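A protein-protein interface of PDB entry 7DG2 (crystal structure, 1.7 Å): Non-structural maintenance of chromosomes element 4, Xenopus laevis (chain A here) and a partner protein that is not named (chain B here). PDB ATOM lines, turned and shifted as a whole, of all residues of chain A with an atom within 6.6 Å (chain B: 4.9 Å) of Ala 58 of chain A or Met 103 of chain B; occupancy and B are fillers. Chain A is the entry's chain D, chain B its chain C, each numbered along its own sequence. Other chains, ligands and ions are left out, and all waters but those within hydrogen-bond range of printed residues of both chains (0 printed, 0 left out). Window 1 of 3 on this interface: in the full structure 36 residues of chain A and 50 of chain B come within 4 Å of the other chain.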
ATOM      1  N   PHE A  12       9.177 -23.851  10.593  1.00  0.00           N
ATOM      2  CA  PHE A  12      10.041 -22.703  10.344  1.00  0.00           C
ATOM      3  C   PHE A  12      11.509 -23.052  10.557  1.00  0.00           C
ATOM      4  O   PHE A  12      12.349 -22.757   9.702  1.00  0.00           O
ATOM      5  CB  PHE A  12       9.616 -21.544  11.245  1.00  0.00           C
ATOM      6  CG  PHE A  12      10.366 -20.255  11.007  1.00  0.00           C
ATOM      7  CD1 PHE A  12      10.495 -19.727   9.734  1.00  0.00           C
ATOM      8  CD2 PHE A  12      10.870 -19.535  12.082  1.00  0.00           C
ATOM      9  CE1 PHE A  12      11.160 -18.523   9.528  1.00  0.00           C
ATOM     10  CE2 PHE A  12      11.534 -18.329  11.890  1.00  0.00           C
ATOM     11  CZ  PHE A  12      11.682 -17.823  10.606  1.00  0.00           C
ATOM     12  N   LYS A  53      25.195 -16.704   5.966  1.00  0.00           N
ATOM     13  CA  LYS A  53      24.285 -16.853   4.832  1.00  0.00           C
ATOM     14  C   LYS A  53      22.904 -16.317   5.177  1.00  0.00           C
ATOM     15  O   LYS A  53      22.297 -15.564   4.403  1.00  0.00           O
ATOM     16  CB  LYS A  53      24.191 -18.323   4.416  1.00  0.00           C
ATOM     17  CG  LYS A  53      25.382 -18.848   3.605  1.00  0.00           C
ATOM     18  CD  LYS A  53      24.972 -20.006   2.680  1.00  0.00           C
ATOM     19  CE  LYS A  53      24.810 -21.332   3.427  1.00  0.00           C
ATOM     20  NZ  LYS A  53      26.108 -22.058   3.637  1.00  0.00           N
ATOM     21  N   LEU A  54      22.397 -16.690   6.353  1.00  0.00           N
ATOM     22  CA  LEU A  54      21.092 -16.209   6.788  1.00  0.00           C
ATOM     23  C   LEU A  54      21.104 -14.702   6.997  1.00  0.00           C
ATOM     24  O   LEU A  54      20.177 -14.000   6.580  1.00  0.00           O
ATOM     25  CB  LEU A  54      20.684 -16.939   8.073  1.00  0.00           C
ATOM     26  CG  LEU A  54      19.235 -16.789   8.533  1.00  0.00           C
ATOM     27  CD1 LEU A  54      18.308 -17.308   7.450  1.00  0.00           C
ATOM     28  CD2 LEU A  54      19.004 -17.551   9.833  1.00  0.00           C
ATOM     29  N   GLY A  55      22.151 -14.182   7.633  1.00  0.00           N
ATOM     30  CA  GLY A  55      22.221 -12.755   7.874  1.00  0.00           C
ATOM     31  C   GLY A  55      22.302 -11.930   6.604  1.00  0.00           C
ATOM     32  O   GLY A  55      21.769 -10.828   6.554  1.00  0.00           O
ATOM     33  N   SER A  56      22.993 -12.433   5.580  1.00  0.00           N
ATOM     34  CA  SER A  56      23.062 -11.701   4.319  1.00  0.00           C
ATOM     35  C   SER A  56      21.696 -11.611   3.661  1.00  0.00           C
ATOM     36  O   SER A  56      21.354 -10.580   3.063  1.00  0.00           O
ATOM     37  CB  SER A  56      24.064 -12.366   3.387  1.00  0.00           C
ATOM     38  OG  SER A  56      25.371 -12.134   3.870  1.00  0.00           O
ATOM     39  N   GLU A  57      20.897 -12.669   3.766  1.00  0.00           N
ATOM     40  CA  GLU A  57      19.518 -12.580   3.297  1.00  0.00           C
ATOM     41  C   GLU A  57      18.738 -11.568   4.130  1.00  0.00           C
ATOM     42  O   GLU A  57      18.082 -10.675   3.592  1.00  0.00           O
ATOM     43  CB  GLU A  57      18.863 -13.962   3.347  1.00  0.00           C
ATOM     44  CG  GLU A  57      17.399 -14.000   2.899  1.00  0.00           C
ATOM     45  CD  GLU A  57      17.208 -13.616   1.439  1.00  0.00           C
ATOM     46  OE1 GLU A  57      18.144 -13.823   0.638  1.00  0.00           O
ATOM     47  OE2 GLU A  57      16.116 -13.108   1.095  1.00  0.00           O
ATOM     48  N   ALA A  58      18.855 -11.661   5.456  1.00  0.00           N
ATOM     49  CA  ALA A  58      18.086 -10.790   6.343  1.00  0.00           C
ATOM     50  C   ALA A  58      18.393  -9.304   6.142  1.00  0.00           C
ATOM     51  O   ALA A  58      17.502  -8.468   6.310  1.00  0.00           O
ATOM     52  CB  ALA A  58      18.348 -11.203   7.794  1.00  0.00           C
ATOM     53  N   GLU A  59      19.636  -8.945   5.777  1.00  0.00           N
ATOM     54  CA  GLU A  59      19.989  -7.528   5.613  1.00  0.00           C
ATOM     55  C   GLU A  59      19.157  -6.843   4.549  1.00  0.00           C
ATOM     56  O   GLU A  59      18.941  -5.624   4.610  1.00  0.00           O
ATOM     57  CB  GLU A  59      21.471  -7.374   5.239  1.00  0.00           C
ATOM     58  CG  GLU A  59      22.450  -7.537   6.388  1.00  0.00           C
ATOM     59  CD  GLU A  59      22.689  -6.255   7.187  1.00  0.00           C
ATOM     60  OE1 GLU A  59      21.873  -5.299   7.110  1.00  0.00           O
ATOM     61  OE2 GLU A  59      23.707  -6.214   7.913  1.00  0.00           O
ATOM     62  N   ASN A  60      18.714  -7.590   3.545  1.00  0.00           N
ATOM     63  CA  ASN A  60      17.948  -6.974   2.482  1.00  0.00           C
ATOM     64  C   ASN A  60      16.562  -6.564   2.939  1.00  0.00           C
ATOM     65  O   ASN A  60      15.851  -5.889   2.184  1.00  0.00           O
ATOM     66  CB  ASN A  60      17.900  -7.932   1.290  1.00  0.00           C
ATOM     67  CG  ASN A  60      19.290  -8.211   0.740  1.00  0.00           C
ATOM     68  OD1 ASN A  60      20.179  -7.361   0.844  1.00  0.00           O
ATOM     69  ND2 ASN A  60      19.500  -9.403   0.192  1.00  0.00           N
ATOM     70  N   TYR A  61      16.178  -6.928   4.165  1.00  0.00           N
ATOM     71  CA  TYR A  61      14.890  -6.554   4.726  1.00  0.00           C
ATOM     72  C   TYR A  61      15.000  -5.441   5.753  1.00  0.00           C
ATOM     73  O   TYR A  61      13.971  -4.995   6.271  1.00  0.00           O
ATOM     74  CB  TYR A  61      14.224  -7.773   5.369  1.00  0.00           C
ATOM     75  CG  TYR A  61      14.015  -8.910   4.404  1.00  0.00           C
ATOM     76  CD1 TYR A  61      15.041  -9.795   4.111  1.00  0.00           C
ATOM     77  CD2 TYR A  61      12.792  -9.101   3.788  1.00  0.00           C
ATOM     78  CE1 TYR A  61      14.858 -10.836   3.215  1.00  0.00           C
ATOM     79  CE2 TYR A  61      12.599 -10.150   2.897  1.00  0.00           C
ATOM     80  CZ  TYR A  61      13.627 -11.011   2.623  1.00  0.00           C
ATOM     81  OH  TYR A  61      13.434 -12.043   1.724  1.00  0.00           O
ATOM     82  N   PHE A  62      16.213  -4.993   6.062  1.00  0.00           N
ATOM     83  CA  PHE A  62      16.456  -3.932   7.025  1.00  0.00           C
ATOM     84  C   PHE A  62      16.982  -2.693   6.310  1.00  0.00           C
ATOM     85  O   PHE A  62      17.458  -2.760   5.174  1.00  0.00           O
ATOM     86  CB  PHE A  62      17.462  -4.371   8.090  1.00  0.00           C
ATOM     87  CG  PHE A  62      16.873  -5.242   9.168  1.00  0.00           C
ATOM     88  CD1 PHE A  62      16.470  -6.534   8.891  1.00  0.00           C
ATOM     89  CD2 PHE A  62      16.739  -4.769  10.461  1.00  0.00           C
ATOM     90  CE1 PHE A  62      15.930  -7.341   9.882  1.00  0.00           C
ATOM     91  CE2 PHE A  62      16.205  -5.573  11.453  1.00  0.00           C
ATOM     92  CZ  PHE A  62      15.808  -6.857  11.165  1.00  0.00           C
ATOM     93  N   LEU B  99      22.409 -10.318  12.631  1.00  0.00           N
ATOM     94  CA  LEU B  99      21.126  -9.923  12.063  1.00  0.00           C
ATOM     95  C   LEU B  99      20.318 -11.136  11.628  1.00  0.00           C
ATOM     96  O   LEU B  99      19.085 -11.114  11.705  1.00  0.00           O
ATOM     97  CB  LEU B  99      21.330  -8.970  10.875  1.00  0.00           C
ATOM     98  CG  LEU B  99      20.053  -8.257  10.449  1.00  0.00           C
ATOM     99  CD1 LEU B  99      19.682  -7.201  11.490  1.00  0.00           C
ATOM    100  CD2 LEU B  99      20.216  -7.632   9.094  1.00  0.00           C
ATOM    101  N   GLY B 100      20.991 -12.195  11.166  1.00  0.00           N
ATOM    102  CA  GLY B 100      20.287 -13.440  10.902  1.00  0.00           C
ATOM    103  C   GLY B 100      19.566 -13.948  12.138  1.00  0.00           C
ATOM    104  O   GLY B 100      18.388 -14.315  12.082  1.00  0.00           O
ATOM    105  N   LEU B 101      20.260 -13.957  13.279  1.00  0.00           N
ATOM    106  CA  LEU B 101      19.630 -14.415  14.517  1.00  0.00           C
ATOM    107  C   LEU B 101      18.484 -13.495  14.914  1.00  0.00           C
ATOM    108  O   LEU B 101      17.387 -13.957  15.255  1.00  0.00           O
ATOM    109  CB  LEU B 101      20.663 -14.506  15.640  1.00  0.00           C
ATOM    110  CG  LEU B 101      20.078 -14.791  17.022  1.00  0.00           C
ATOM    111  CD1 LEU B 101      19.337 -16.115  17.029  1.00  0.00           C
ATOM    112  CD2 LEU B 101      21.172 -14.796  18.083  1.00  0.00           C
ATOM    113  N   LEU B 102      18.712 -12.181  14.859  1.00  0.00           N
ATOM    114  CA  LEU B 102      17.657 -11.250  15.236  1.00  0.00           C
ATOM    115  C   LEU B 102      16.429 -11.426  14.359  1.00  0.00           C
ATOM    116  O   LEU B 102      15.293 -11.390  14.850  1.00  0.00           O
ATOM    117  CB  LEU B 102      18.167  -9.810  15.156  1.00  0.00           C
ATOM    118  CG  LEU B 102      17.076  -8.745  15.330  1.00  0.00           C
ATOM    119  CD1 LEU B 102      16.518  -8.774  16.746  1.00  0.00           C
ATOM    120  CD2 LEU B 102      17.669  -7.387  15.010  1.00  0.00           C
ATOM    121  N   MET B 103      16.631 -11.628  13.054  1.00  0.00           N
ATOM    122  CA  MET B 103      15.481 -11.743  12.162  1.00  0.00           C
ATOM    123  C   MET B 103      14.638 -12.969  12.499  1.00  0.00           C
ATOM    124  O   MET B 103      13.404 -12.936  12.405  1.00  0.00           O
ATOM    125  CB  MET B 103      15.955 -11.806  10.711  1.00  0.00           C
ATOM    126  CG  MET B 103      14.843 -12.097   9.710  1.00  0.00           C
ATOM    127  SD  MET B 103      13.610 -10.784   9.620  1.00  0.00           S
ATOM    128  CE  MET B 103      14.128  -9.939   8.110  1.00  0.00           C
ATOM    129  N   VAL B 104      15.289 -14.057  12.893  1.00  0.00           N
ATOM    130  CA  VAL B 104      14.561 -15.259  13.288  1.00  0.00           C
ATOM    131  C   VAL B 104      13.713 -14.979  14.523  1.00  0.00           C
ATOM    132  O   VAL B 104      12.555 -15.411  14.615  1.00  0.00           O
ATOM    133  CB  VAL B 104      15.556 -16.409  13.518  1.00  0.00           C
ATOM    134  CG1 VAL B 104      14.873 -17.585  14.194  1.00  0.00           C
ATOM    135  CG2 VAL B 104      16.175 -16.830  12.202  1.00  0.00           C
ATOM    136  N   ILE B 105      14.265 -14.229  15.478  1.00  0.00           N
ATOM    137  CA  ILE B 105      13.528 -13.879  16.693  1.00  0.00           C
ATOM    138  C   ILE B 105      12.383 -12.919  16.371  1.00  0.00           C
ATOM    139  O   ILE B 105      11.249 -13.095  16.840  1.00  0.00           O
ATOM    140  CB  ILE B 105      14.487 -13.289  17.746  1.00  0.00           C
ATOM    141  CG1 ILE B 105      15.504 -14.339  18.187  1.00  0.00           C
ATOM    142  CG2 ILE B 105      13.717 -12.748  18.943  1.00  0.00           C
ATOM    143  CD1 ILE B 105      16.616 -13.759  19.070  1.00  0.00           C
ATOM    144  N   LEU B 106      12.658 -11.881  15.575  1.00  0.00           N
ATOM    145  CA  LEU B 106      11.583 -10.971  15.179  1.00  0.00           C
ATOM    146  C   LEU B 106      10.472 -11.720  14.459  1.00  0.00           C
ATOM    147  O   LEU B 106       9.290 -11.377  14.588  1.00  0.00           O
ATOM    148  CB  LEU B 106      12.124  -9.859  14.270  1.00  0.00           C
ATOM    149  CG  LEU B 106      13.094  -8.844  14.898  1.00  0.00           C
ATOM    150  CD1 LEU B 106      13.644  -7.917  13.816  1.00  0.00           C
ATOM    151  CD2 LEU B 106      12.401  -8.024  15.970  1.00  0.00           C
ATOM    152  N   SER B 107      10.845 -12.719  13.658  1.00  0.00           N
ATOM    153  CA  SER B 107       9.865 -13.499  12.913  1.00  0.00           C
ATOM    154  C   SER B 107       8.914 -14.220  13.855  1.00  0.00           C
ATOM    155  O   SER B 107       7.693 -14.149  13.687  1.00  0.00           O
ATOM    156  CB  SER B 107      10.566 -14.504  11.997  1.00  0.00           C
ATOM    157  OG  SER B 107      11.271 -13.846  10.947  1.00  0.00           O
ATOM    158  N   THR B 181      13.041  -2.167   9.974  1.00  0.00           N
ATOM    159  CA  THR B 181      12.319  -3.122   9.128  1.00  0.00           C
ATOM    160  C   THR B 181      10.824  -2.857   9.315  1.00  0.00           C
ATOM    161  O   THR B 181      10.406  -1.784   9.759  1.00  0.00           O
ATOM    162  CB  THR B 181      12.780  -4.569   9.427  1.00  0.00           C
ATOM    163  OG1 THR B 181      12.283  -5.462   8.416  1.00  0.00           O
ATOM    164  CG2 THR B 181      12.326  -5.059  10.808  1.00  0.00           C
ATOM    165  N   VAL B 186       9.214  -8.487   7.299  1.00  0.00           N
ATOM    166  CA  VAL B 186       9.505  -9.722   8.026  1.00  0.00           C
ATOM    167  C   VAL B 186       8.619 -10.860   7.512  1.00  0.00           C
ATOM    168  O   VAL B 186       9.073 -12.002   7.356  1.00  0.00           O
ATOM    169  CB  VAL B 186       9.347  -9.501   9.540  1.00  0.00           C
ATOM    170  CG1 VAL B 186       9.443 -10.832  10.281  1.00  0.00           C
ATOM    171  CG2 VAL B 186      10.433  -8.535  10.048  1.00  0.00           C
ATOM    172  N   PHE B 189      10.190 -12.164   4.456  1.00  0.00           N
ATOM    173  CA  PHE B 189      11.302 -13.044   4.780  1.00  0.00           C
ATOM    174  C   PHE B 189      10.807 -14.422   5.199  1.00  0.00           C
ATOM    175  O   PHE B 189      11.286 -15.444   4.699  1.00  0.00           O
ATOM    176  CB  PHE B 189      12.145 -12.414   5.893  1.00  0.00           C
ATOM    177  CG  PHE B 189      13.184 -13.334   6.457  1.00  0.00           C
ATOM    178  CD1 PHE B 189      14.438 -13.425   5.868  1.00  0.00           C
ATOM    179  CD2 PHE B 189      12.912 -14.106   7.581  1.00  0.00           C
ATOM    180  CE1 PHE B 189      15.403 -14.274   6.390  1.00  0.00           C
ATOM    181  CE2 PHE B 189      13.867 -14.958   8.100  1.00  0.00           C
ATOM    182  CZ  PHE B 189      15.115 -15.041   7.504  1.00  0.00           C
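O of Met 103 of chain B sits at hydrogen-bond distance from OG of Ser 107 of chain B, 2.7 Å away.
The side-chain hydroxyl (OH) of Tyr 61 of chain A is in hydrogen-bond range of the side-chain carboxylate (OE2) of Glu 57 of chain A, at 3.0 Å.
The side-chain hydroxyl (OG1) of Thr 181 of chain B is in hydrogen-bond range of the backbone carbonyl oxygen (O) of Tyr 61 of chain A (2.8 Å).
Among the printed residues, pairs that only touch across the chains: Phe 12 of chain A with Ser 107 of chain B (3.8 Å), Leu 54 of chain A with Gly 100 of chain B (3.99 Å), Leu 54 of chain A with Val 104 of chain B (3.8 Å), Leu 54 of chain A with Phe 189 of chain B (3.9 Å), Gly 55 of chain A with Gly 100 of chain B (3.6 Å), Ala 58 of chain A with Leu 99 of chain B (3.9 Å), Ala 58 of chain A with Met 103 of chain B (3.8 Å), Glu 59 of chain A with Leu 99 of chain B (3.4 Å), Tyr 61 of chain A with Met 103 of chain B (3.5 Å), Tyr 61 of chain A with Phe 189 of chain B (3.5 Å), Phe 62 of chain A with Leu 99 of chain B (3.8 Å), Phe 62 of chain A with Met 103 of chain B (3.6 Å), Phe 62 of chain A with Leu 106 of chain B (3.6 Å) and Phe 62 of chain A with Thr 181 of chain B (3.9 Å).
Ala 58 of chain A touches just these residues of chain B: Leu 99 and Met 103.
Of chain A, only Ala 58, Tyr 61 and Phe 62 come within 4 Å of Met 103 of chain B.
Of the printed residues of chain A, Leu 106 of chain B touches Phe 62 (3.6 Å).
Printed residues of chain B within 4 Å of Phe 12 of chain A: Ser 107 (3.8 Å).
Printed residues of chain A within 4 Å of Ser 107 of chain B: Phe 12 (3.8 Å).
Of the printed residues of chain B, Glu 59 of chain A touches Leu 99.
Of the printed residues of chain A, Gly 100 of chain B touches Leu 54 and Gly 55.
Asn 60 of chain A touches none of the printed residues of chain B.
Ser 56 of chain A touches none of the printed residues of chain B.
The nearest residue of chain A that does not touch Met 103 of chain B is Phe 12 of chain A (5.5 Å).
Hydrophobic or aromatic side chains of chain B within 4 Å of the printed part of chain A: Leu 99, Met 103, Val 104, Leu 106 and Phe 189.
Of the 11 printed residues of chain A, 7 touch a printed residue of chain B.
Hydrophobic or aromatic side chains of chain A within 4 Å of the printed part of chain B: Phe 12, Leu 54, Ala 58, Tyr 61 and Phe 62.
Along chain A the printed residues that touch a printed residue of chain B span positions 12 to 62.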
